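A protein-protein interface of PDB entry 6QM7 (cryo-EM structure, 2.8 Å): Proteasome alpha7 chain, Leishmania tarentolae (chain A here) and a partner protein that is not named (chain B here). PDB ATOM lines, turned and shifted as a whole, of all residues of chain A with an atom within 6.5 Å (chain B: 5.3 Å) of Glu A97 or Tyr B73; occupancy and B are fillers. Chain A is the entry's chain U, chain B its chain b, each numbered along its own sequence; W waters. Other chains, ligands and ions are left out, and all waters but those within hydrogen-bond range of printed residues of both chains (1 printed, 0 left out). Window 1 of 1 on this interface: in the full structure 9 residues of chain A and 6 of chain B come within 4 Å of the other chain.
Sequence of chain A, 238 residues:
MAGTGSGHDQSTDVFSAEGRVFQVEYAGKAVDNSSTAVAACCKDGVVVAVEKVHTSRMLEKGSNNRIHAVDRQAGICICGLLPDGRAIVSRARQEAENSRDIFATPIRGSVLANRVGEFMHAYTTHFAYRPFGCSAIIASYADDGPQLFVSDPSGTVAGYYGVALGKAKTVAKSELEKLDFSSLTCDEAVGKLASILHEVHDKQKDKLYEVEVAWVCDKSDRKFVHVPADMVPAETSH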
ATOM      1  N   HIS A  68     -19.078 -30.026   8.599  1.00  0.00           N
ATOM      2  CA  HIS A  68     -18.507 -29.798   9.942  1.00  0.00           C
ATOM      3  C   HIS A  68     -19.574 -30.025  10.995  1.00  0.00           C
ATOM      4  O   HIS A  68     -20.679 -29.504  10.826  1.00  0.00           O
ATOM      5  CB  HIS A  68     -17.957 -28.382  10.050  1.00  0.00           C
ATOM      6  CG  HIS A  68     -16.943 -28.092   9.010  1.00  0.00           C
ATOM      7  ND1 HIS A  68     -15.644 -28.529   9.112  1.00  0.00           N
ATOM      8  CD2 HIS A  68     -17.054 -27.454   7.829  1.00  0.00           C
ATOM      9  CE1 HIS A  68     -14.985 -28.152   8.038  1.00  0.00           C
ATOM     10  NE2 HIS A  68     -15.829 -27.484   7.233  1.00  0.00           N
ATOM     11  N   ALA A  69     -19.235 -30.764  12.039  1.00  0.00           N
ATOM     12  CA  ALA A  69     -20.136 -30.987  13.179  1.00  0.00           C
ATOM     13  C   ALA A  69     -20.266 -29.658  13.918  1.00  0.00           C
ATOM     14  O   ALA A  69     -19.238 -29.073  14.296  1.00  0.00           O
ATOM     15  CB  ALA A  69     -19.605 -32.087  14.067  1.00  0.00           C
ATOM     16  N   VAL A  70     -21.490 -29.190  14.084  1.00  0.00           N
ATOM     17  CA  VAL A  70     -21.811 -27.959  14.844  1.00  0.00           C
ATOM     18  C   VAL A  70     -22.053 -28.371  16.297  1.00  0.00           C
ATOM     19  O   VAL A  70     -21.623 -27.646  17.219  1.00  0.00           O
ATOM     20  CB  VAL A  70     -23.027 -27.294  14.190  1.00  0.00           C
ATOM     21  CG1 VAL A  70     -23.802 -26.445  15.165  1.00  0.00           C
ATOM     22  CG2 VAL A  70     -22.626 -26.483  12.977  1.00  0.00           C
ATOM     23  N   ASP A  71     -22.742 -29.493  16.492  1.00  0.00           N
ATOM     24  CA  ASP A  71     -22.972 -30.117  17.816  1.00  0.00           C
ATOM     25  C   ASP A  71     -23.027 -31.623  17.609  1.00  0.00           C
ATOM     26  O   ASP A  71     -22.871 -32.031  16.465  1.00  0.00           O
ATOM     27  CB  ASP A  71     -24.272 -29.618  18.436  1.00  0.00           C
ATOM     28  CG  ASP A  71     -24.271 -29.563  19.959  1.00  0.00           C
ATOM     29  OD1 ASP A  71     -23.437 -30.276  20.587  1.00  0.00           O
ATOM     30  OD2 ASP A  71     -25.129 -28.811  20.525  1.00  0.00           O
ATOM     31  N   ARG A  86     -16.774 -21.412   7.229  1.00  0.00           N
ATOM     32  CA  ARG A  86     -16.178 -21.843   8.513  1.00  0.00           C
ATOM     33  C   ARG A  86     -16.462 -20.795   9.595  1.00  0.00           C
ATOM     34  O   ARG A  86     -16.498 -21.190  10.765  1.00  0.00           O
ATOM     35  CB  ARG A  86     -14.702 -22.182   8.307  1.00  0.00           C
ATOM     36  CG  ARG A  86     -14.527 -23.377   7.382  1.00  0.00           C
ATOM     37  CD  ARG A  86     -13.361 -24.262   7.741  1.00  0.00           C
ATOM     38  NE  ARG A  86     -13.570 -24.862   9.048  1.00  0.00           N
ATOM     39  CZ  ARG A  86     -12.678 -25.611   9.681  1.00  0.00           C
ATOM     40  NH1 ARG A  86     -12.963 -26.096  10.879  1.00  0.00           N
ATOM     41  NH2 ARG A  86     -11.508 -25.871   9.124  1.00  0.00           N
ATOM     42  N   SER A  90     -18.290 -21.819  12.872  1.00  0.00           N
ATOM     43  CA  SER A  90     -17.751 -21.366  14.178  1.00  0.00           C
ATOM     44  C   SER A  90     -18.851 -20.681  14.977  1.00  0.00           C
ATOM     45  O   SER A  90     -18.899 -20.915  16.202  1.00  0.00           O
ATOM     46  CB  SER A  90     -16.550 -20.499  14.040  1.00  0.00           C
ATOM     47  OG  SER A  90     -15.409 -21.322  13.873  1.00  0.00           O
ATOM     48  N   ALA A  92     -22.268 -21.184  14.477  1.00  0.00           N
ATOM     49  CA  ALA A  92     -23.300 -22.219  14.715  1.00  0.00           C
ATOM     50  C   ALA A  92     -22.895 -23.041  15.936  1.00  0.00           C
ATOM     51  O   ALA A  92     -23.771 -23.425  16.707  1.00  0.00           O
ATOM     52  CB  ALA A  92     -23.472 -23.083  13.498  1.00  0.00           C
ATOM     53  N   ARG A  93     -21.594 -23.284  16.075  1.00  0.00           N
ATOM     54  CA  ARG A  93     -20.968 -23.964  17.232  1.00  0.00           C
ATOM     55  C   ARG A  93     -21.180 -23.139  18.491  1.00  0.00           C
ATOM     56  O   ARG A  93     -21.711 -23.688  19.439  1.00  0.00           O
ATOM     57  CB  ARG A  93     -19.490 -24.189  16.944  1.00  0.00           C
ATOM     58  CG  ARG A  93     -19.303 -25.340  15.978  1.00  0.00           C
ATOM     59  CD  ARG A  93     -17.897 -25.458  15.472  1.00  0.00           C
ATOM     60  NE  ARG A  93     -17.755 -26.638  14.648  1.00  0.00           N
ATOM     61  CZ  ARG A  93     -16.628 -26.982  14.063  1.00  0.00           C
ATOM     62  NH1 ARG A  93     -15.548 -26.235  14.220  1.00  0.00           N
ATOM     63  NH2 ARG A  93     -16.576 -28.075  13.326  1.00  0.00           N
ATOM     64  N   GLN A  94     -20.815 -21.864  18.453  1.00  0.00           N
ATOM     65  CA  GLN A  94     -20.990 -20.917  19.578  1.00  0.00           C
ATOM     66  C   GLN A  94     -22.447 -20.962  20.054  1.00  0.00           C
ATOM     67  O   GLN A  94     -22.654 -20.905  21.271  1.00  0.00           O
ATOM     68  CB  GLN A  94     -20.558 -19.510  19.171  1.00  0.00           C
ATOM     69  CG  GLN A  94     -20.275 -18.585  20.348  1.00  0.00           C
ATOM     70  CD  GLN A  94     -20.110 -17.147  19.907  1.00  0.00           C
ATOM     71  OE1 GLN A  94     -20.936 -16.281  20.207  1.00  0.00           O
ATOM     72  NE2 GLN A  94     -19.044 -16.882  19.160  1.00  0.00           N
ATOM     73  N   GLU A  95     -23.417 -21.078  19.147  1.00  0.00           N
ATOM     74  CA  GLU A  95     -24.866 -21.062  19.483  1.00  0.00           C
ATOM     75  C   GLU A  95     -25.265 -22.409  20.071  1.00  0.00           C
ATOM     76  O   GLU A  95     -26.052 -22.432  21.035  1.00  0.00           O
ATOM     77  CB  GLU A  95     -25.713 -20.772  18.244  1.00  0.00           C
ATOM     78  CG  GLU A  95     -25.435 -19.408  17.632  1.00  0.00           C
ATOM     79  CD  GLU A  95     -25.868 -18.193  18.456  1.00  0.00           C
ATOM     80  OE1 GLU A  95     -26.497 -18.374  19.531  1.00  0.00           O
ATOM     81  OE2 GLU A  95     -25.586 -17.053  18.004  1.00  0.00           O
ATOM     82  N   ALA A  96     -24.771 -23.484  19.467  1.00  0.00           N
ATOM     83  CA  ALA A  96     -24.995 -24.871  19.910  1.00  0.00           C
ATOM     84  C   ALA A  96     -24.457 -25.048  21.329  1.00  0.00           C
ATOM     85  O   ALA A  96     -25.112 -25.747  22.117  1.00  0.00           O
ATOM     86  CB  ALA A  96     -24.343 -25.827  18.948  1.00  0.00           C
ATOM     87  N   GLU A  97     -23.310 -24.444  21.633  1.00  0.00           N
ATOM     88  CA  GLU A  97     -22.693 -24.568  22.974  1.00  0.00           C
ATOM     89  C   GLU A  97     -23.336 -23.587  23.957  1.00  0.00           C
ATOM     90  O   GLU A  97     -23.355 -23.926  25.130  1.00  0.00           O
ATOM     91  CB  GLU A  97     -21.158 -24.550  22.951  1.00  0.00           C
ATOM     92  CG  GLU A  97     -20.430 -23.373  22.329  1.00  0.00           C
ATOM     93  CD  GLU A  97     -19.030 -23.725  21.794  1.00  0.00           C
ATOM     94  OE1 GLU A  97     -18.352 -22.841  21.200  1.00  0.00           O
ATOM     95  OE2 GLU A  97     -18.606 -24.888  21.960  1.00  0.00           O
ATOM     96  N   ASN A  98     -23.908 -22.474  23.517  1.00  0.00           N
ATOM     97  CA  ASN A  98     -24.734 -21.615  24.401  1.00  0.00           C
ATOM     98  C   ASN A  98     -26.015 -22.354  24.765  1.00  0.00           C
ATOM     99  O   ASN A  98     -26.485 -22.152  25.878  1.00  0.00           O
ATOM    100  CB  ASN A  98     -25.082 -20.257  23.789  1.00  0.00           C
ATOM    101  CG  ASN A  98     -23.889 -19.325  23.729  1.00  0.00           C
ATOM    102  OD1 ASN A  98     -22.859 -19.567  24.359  1.00  0.00           O
ATOM    103  ND2 ASN A  98     -24.008 -18.268  22.939  1.00  0.00           N
ATOM    104  N   SER A  99     -26.574 -23.172  23.883  1.00  0.00           N
ATOM    105  CA  SER A  99     -27.820 -23.918  24.198  1.00  0.00           C
ATOM    106  C   SER A  99     -27.541 -24.902  25.323  1.00  0.00           C
ATOM    107  O   SER A  99     -28.384 -25.019  26.203  1.00  0.00           O
ATOM    108  CB  SER A  99     -28.411 -24.621  23.006  1.00  0.00           C
ATOM    109  OG  SER A  99     -29.796 -24.871  23.218  1.00  0.00           O
ATOM    110  N   ARG A 100     -26.389 -25.567  25.292  1.00  0.00           N
ATOM    111  CA  ARG A 100     -26.007 -26.592  26.291  1.00  0.00           C
ATOM    112  C   ARG A 100     -25.483 -25.913  27.555  1.00  0.00           C
ATOM    113  O   ARG A 100     -25.797 -26.408  28.646  1.00  0.00           O
ATOM    114  CB  ARG A 100     -25.004 -27.566  25.683  1.00  0.00           C
ATOM    115  CG  ARG A 100     -25.573 -28.293  24.477  1.00  0.00           C
ATOM    116  CD  ARG A 100     -24.632 -29.337  23.911  1.00  0.00           C
ATOM    117  NE  ARG A 100     -25.178 -30.623  24.264  1.00  0.00           N
ATOM    118  CZ  ARG A 100     -25.758 -31.479  23.446  1.00  0.00           C
ATOM    119  NH1 ARG A 100     -26.219 -32.605  23.950  1.00  0.00           N
ATOM    120  NH2 ARG A 100     -25.872 -31.256  22.148  1.00  0.00           N
ATOM    121  N   ASP A 101     -24.724 -24.831  27.422  1.00  0.00           N
ATOM    122  CA  ASP A 101     -24.127 -24.129  28.582  1.00  0.00           C
ATOM    123  C   ASP A 101     -25.236 -23.427  29.365  1.00  0.00           C
ATOM    124  O   ASP A 101     -25.309 -23.626  30.601  1.00  0.00           O
ATOM    125  CB  ASP A 101     -23.009 -23.182  28.149  1.00  0.00           C
ATOM    126  CG  ASP A 101     -21.779 -23.870  27.552  1.00  0.00           C
ATOM    127  OD1 ASP A 101     -21.821 -25.117  27.336  1.00  0.00           O
ATOM    128  OD2 ASP A 101     -20.777 -23.146  27.278  1.00  0.00           O
ATOM    129  N   ILE A 102     -26.100 -22.694  28.675  1.00  0.00           N
ATOM    130  CA  ILE A 102     -27.067 -21.757  29.314  1.00  0.00           C
ATOM    131  C   ILE A 102     -28.399 -22.469  29.559  1.00  0.00           C
ATOM    132  O   ILE A 102     -28.917 -22.335  30.673  1.00  0.00           O
ATOM    133  CB  ILE A 102     -27.200 -20.473  28.477  1.00  0.00           C
ATOM    134  CG1 ILE A 102     -25.874 -19.708  28.449  1.00  0.00           C
ATOM    135  CG2 ILE A 102     -28.335 -19.598  28.979  1.00  0.00           C
ATOM    136  CD1 ILE A 102     -25.769 -18.717  27.306  1.00  0.00           C
ATOM    137  N   ILE A 107     -29.422 -27.664  21.164  1.00  0.00           N
ATOM    138  CA  ILE A 107     -30.104 -26.658  20.313  1.00  0.00           C
ATOM    139  C   ILE A 107     -30.955 -27.430  19.309  1.00  0.00           C
ATOM    140  O   ILE A 107     -30.450 -28.417  18.724  1.00  0.00           O
ATOM    141  CB  ILE A 107     -29.090 -25.712  19.646  1.00  0.00           C
ATOM    142  CG1 ILE A 107     -29.787 -24.441  19.156  1.00  0.00           C
ATOM    143  CG2 ILE A 107     -28.279 -26.417  18.550  1.00  0.00           C
ATOM    144  CD1 ILE A 107     -28.833 -23.361  18.694  1.00  0.00           C
ATOM    145  N   GLU B  68     -14.881 -32.525  24.686  1.00  0.00           N
ATOM    146  CA  GLU B  68     -15.834 -32.982  23.631  1.00  0.00           C
ATOM    147  C   GLU B  68     -15.772 -32.014  22.452  1.00  0.00           C
ATOM    148  O   GLU B  68     -15.715 -32.486  21.310  1.00  0.00           O
ATOM    149  CB  GLU B  68     -17.283 -33.124  24.118  1.00  0.00           C
ATOM    150  CG  GLU B  68     -17.708 -34.573  24.387  1.00  0.00           C
ATOM    151  CD  GLU B  68     -17.931 -34.940  25.852  1.00  0.00           C
ATOM    152  OE1 GLU B  68     -17.102 -35.706  26.415  1.00  0.00           O
ATOM    153  OE2 GLU B  68     -18.941 -34.461  26.435  1.00  0.00           O
ATOM    154  N   ARG B  69     -15.791 -30.717  22.737  1.00  0.00           N
ATOM    155  CA  ARG B  69     -15.677 -29.641  21.728  1.00  0.00           C
ATOM    156  C   ARG B  69     -14.433 -29.860  20.864  1.00  0.00           C
ATOM    157  O   ARG B  69     -14.588 -29.994  19.650  1.00  0.00           O
ATOM    158  CB  ARG B  69     -15.622 -28.271  22.401  1.00  0.00           C
ATOM    159  CG  ARG B  69     -16.928 -27.502  22.315  1.00  0.00           C
ATOM    160  CD  ARG B  69     -18.001 -27.857  23.315  1.00  0.00           C
ATOM    161  NE  ARG B  69     -18.239 -26.761  24.247  1.00  0.00           N
ATOM    162  CZ  ARG B  69     -19.373 -26.558  24.923  1.00  0.00           C
ATOM    163  NH1 ARG B  69     -19.457 -25.533  25.758  1.00  0.00           N
ATOM    164  NH2 ARG B  69     -20.419 -27.363  24.772  1.00  0.00           N
ATOM    165  N   GLN B  70     -13.253 -29.919  21.462  1.00  0.00           N
ATOM    166  CA  GLN B  70     -11.973 -30.046  20.721  1.00  0.00           C
ATOM    167  C   GLN B  70     -12.028 -31.261  19.790  1.00  0.00           C
ATOM    168  O   GLN B  70     -11.574 -31.150  18.650  1.00  0.00           O
ATOM    169  CB  GLN B  70     -10.795 -30.159  21.687  1.00  0.00           C
ATOM    170  CG  GLN B  70      -9.458 -29.818  21.044  1.00  0.00           C
ATOM    171  CD  GLN B  70      -8.314 -30.743  21.393  1.00  0.00           C
ATOM    172  OE1 GLN B  70      -8.488 -31.949  21.611  1.00  0.00           O
ATOM    173  NE2 GLN B  70      -7.114 -30.177  21.406  1.00  0.00           N
ATOM    174  N   LYS B  71     -12.554 -32.382  20.268  1.00  0.00           N
ATOM    175  CA  LYS B  71     -12.603 -33.673  19.535  1.00  0.00           C
ATOM    176  C   LYS B  71     -13.562 -33.543  18.356  1.00  0.00           C
ATOM    177  O   LYS B  71     -13.313 -34.167  17.307  1.00  0.00           O
ATOM    178  CB  LYS B  71     -13.106 -34.766  20.483  1.00  0.00           C
ATOM    179  CG  LYS B  71     -12.999 -36.211  20.001  1.00  0.00           C
ATOM    180  CD  LYS B  71     -14.009 -37.161  20.660  1.00  0.00           C
ATOM    181  CE  LYS B  71     -14.298 -36.826  22.113  1.00  0.00           C
ATOM    182  NZ  LYS B  71     -14.884 -37.968  22.852  1.00  0.00           N
ATOM    183  N   MET B  72     -14.646 -32.800  18.562  1.00  0.00           N
ATOM    184  CA  MET B  72     -15.809 -32.734  17.650  1.00  0.00           C
ATOM    185  C   MET B  72     -15.565 -31.683  16.572  1.00  0.00           C
ATOM    186  O   MET B  72     -15.963 -31.927  15.418  1.00  0.00           O
ATOM    187  CB  MET B  72     -17.065 -32.363  18.434  1.00  0.00           C
ATOM    188  CG  MET B  72     -18.332 -32.354  17.591  1.00  0.00           C
ATOM    189  SD  MET B  72     -19.574 -31.306  18.344  1.00  0.00           S
ATOM    190  CE  MET B  72     -19.719 -32.111  19.937  1.00  0.00           C
ATOM    191  N   TYR B  73     -14.986 -30.551  16.960  1.00  0.00           N
ATOM    192  CA  TYR B  73     -14.777 -29.382  16.076  1.00  0.00           C
ATOM    193  C   TYR B  73     -13.658 -29.704  15.103  1.00  0.00           C
ATOM    194  O   TYR B  73     -13.925 -29.683  13.891  1.00  0.00           O
ATOM    195  CB  TYR B  73     -14.518 -28.107  16.876  1.00  0.00           C
ATOM    196  CG  TYR B  73     -15.705 -27.613  17.671  1.00  0.00           C
ATOM    197  CD1 TYR B  73     -16.929 -28.270  17.644  1.00  0.00           C
ATOM    198  CD2 TYR B  73     -15.619 -26.461  18.440  1.00  0.00           C
ATOM    199  CE1 TYR B  73     -18.012 -27.819  18.375  1.00  0.00           C
ATOM    200  CE2 TYR B  73     -16.700 -25.998  19.178  1.00  0.00           C
ATOM    201  CZ  TYR B  73     -17.903 -26.681  19.148  1.00  0.00           C
ATOM    202  OH  TYR B  73     -18.999 -26.260  19.851  1.00  0.00           O
ATOM    203  N   HIS B  74     -12.479 -30.032  15.614  1.00  0.00           N
ATOM    204  CA  HIS B  74     -11.278 -30.350  14.801  1.00  0.00           C
ATOM    205  C   HIS B  74     -11.115 -31.867  14.765  1.00  0.00           C
ATOM    206  O   HIS B  74     -11.286 -32.485  15.821  1.00  0.00           O
ATOM    207  CB  HIS B  74     -10.069 -29.648  15.396  1.00  0.00           C
ATOM    208  CG  HIS B  74     -10.380 -28.340  16.033  1.00  0.00           C
ATOM    209  ND1 HIS B  74     -10.495 -27.175  15.304  1.00  0.00           N
ATOM    210  CD2 HIS B  74     -10.558 -28.002  17.330  1.00  0.00           C
ATOM    211  CE1 HIS B  74     -10.740 -26.169  16.125  1.00  0.00           C
ATOM    212  NE2 HIS B  74     -10.790 -26.652  17.377  1.00  0.00           N
ATOM    213  N   ASN B  75     -10.802 -32.459  13.614  1.00  0.00           N
ATOM    214  CA  ASN B  75     -10.665 -33.938  13.494  1.00  0.00           C
ATOM    215  C   ASN B  75      -9.300 -34.316  14.070  1.00  0.00           C
ATOM    216  O   ASN B  75      -8.405 -34.685  13.293  1.00  0.00           O
ATOM    217  CB  ASN B  75     -10.955 -34.438  12.072  1.00  0.00           C
ATOM    218  CG  ASN B  75     -12.406 -34.216  11.664  1.00  0.00           C
ATOM    219  OD1 ASN B  75     -12.690 -33.904  10.506  1.00  0.00           O
ATOM    220  ND2 ASN B  75     -13.340 -34.361  12.597  1.00  0.00           N
HETATM  221  O   HOH W   1     -21.781 -28.380  21.971  1.00  0.00           O
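OH of Tyr B73 lies within hydrogen-bond range of OE2 of Glu A97 (2.5 Å). The side-chain carboxylate (OE2) of Glu A97 lies within salt-bridge range of the guanidinium group (NE) of Arg B69, 3.0 Å away. The guanidinium group of Arg B69 lies within salt-bridge range of the side-chain carboxylate of Asp A101. The backbone carbonyl oxygen (O) of Tyr B73 is in hydrogen-bond range of the guanidinium group (NH2) of Arg A93.
Of chain B, only Arg B69 (3.0 Å) and Tyr B73 (2.5 Å) come within 4 Å of Glu A97. Tyr B73 touches just these residues of chain A: Val A70 (3.8 Å), Arg A93 (3.2 Å) and Glu A97 (2.5 Å). Of the printed residues of chain B, Asp A71 touches Met B72 (3.5 Å). Printed residues of chain A within 4 Å of Arg B69: Glu A97 (3.0 Å) and Asp A101 (2.9 Å). Of the printed residues of chain B, Arg A93 touches Tyr B73 (3.2 Å). Printed residues of chain B within 4 Å of Val A70: Tyr B73. Printed residues of chain A within 4 Å of Met B72: Ala A69 (3.8 Å) and Asp A71 (3.5 Å). Asn B75 touches none of the printed residues of chain A. The nearest printed residue of chain B that does not touch Glu A97 is Gln B70 (7.4 Å). The nearest residue of chain A that does not touch Tyr B73 is Ala A69 (4.1 Å). The nearest printed residue of chain B that does not touch Val A70 is Met B72 (4.3 Å).
Of the 18 printed residues of chain A, 6 touch a printed residue of chain B. Hydrophobic or aromatic side chains of chain A within 4 Å of the printed part of chain B: Ala A69. Of the 8 printed residues of chain B, 3 touch a printed residue of chain A.
Met B72 touches Ala A69. CE1 of Tyr B73 touches O of Val A70, at 3.8 Å. C of Asp A71 touches SD of Met B72, 3.5 Å away.
Water W1 lies within hydrogen-bond range of OD1 of Asp A71 (2.9 Å) and NH2 of Arg B69 (3.3 Å).
The side-chain carboxylate of Asp A71 is in salt-bridge range of the guanidinium group of Arg A100, 3.0 Å away. The backbone carbonyl oxygen of Ala A69 lies within hydrogen-bond range of the guanidinium group of Arg A93 (2.9 Å).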
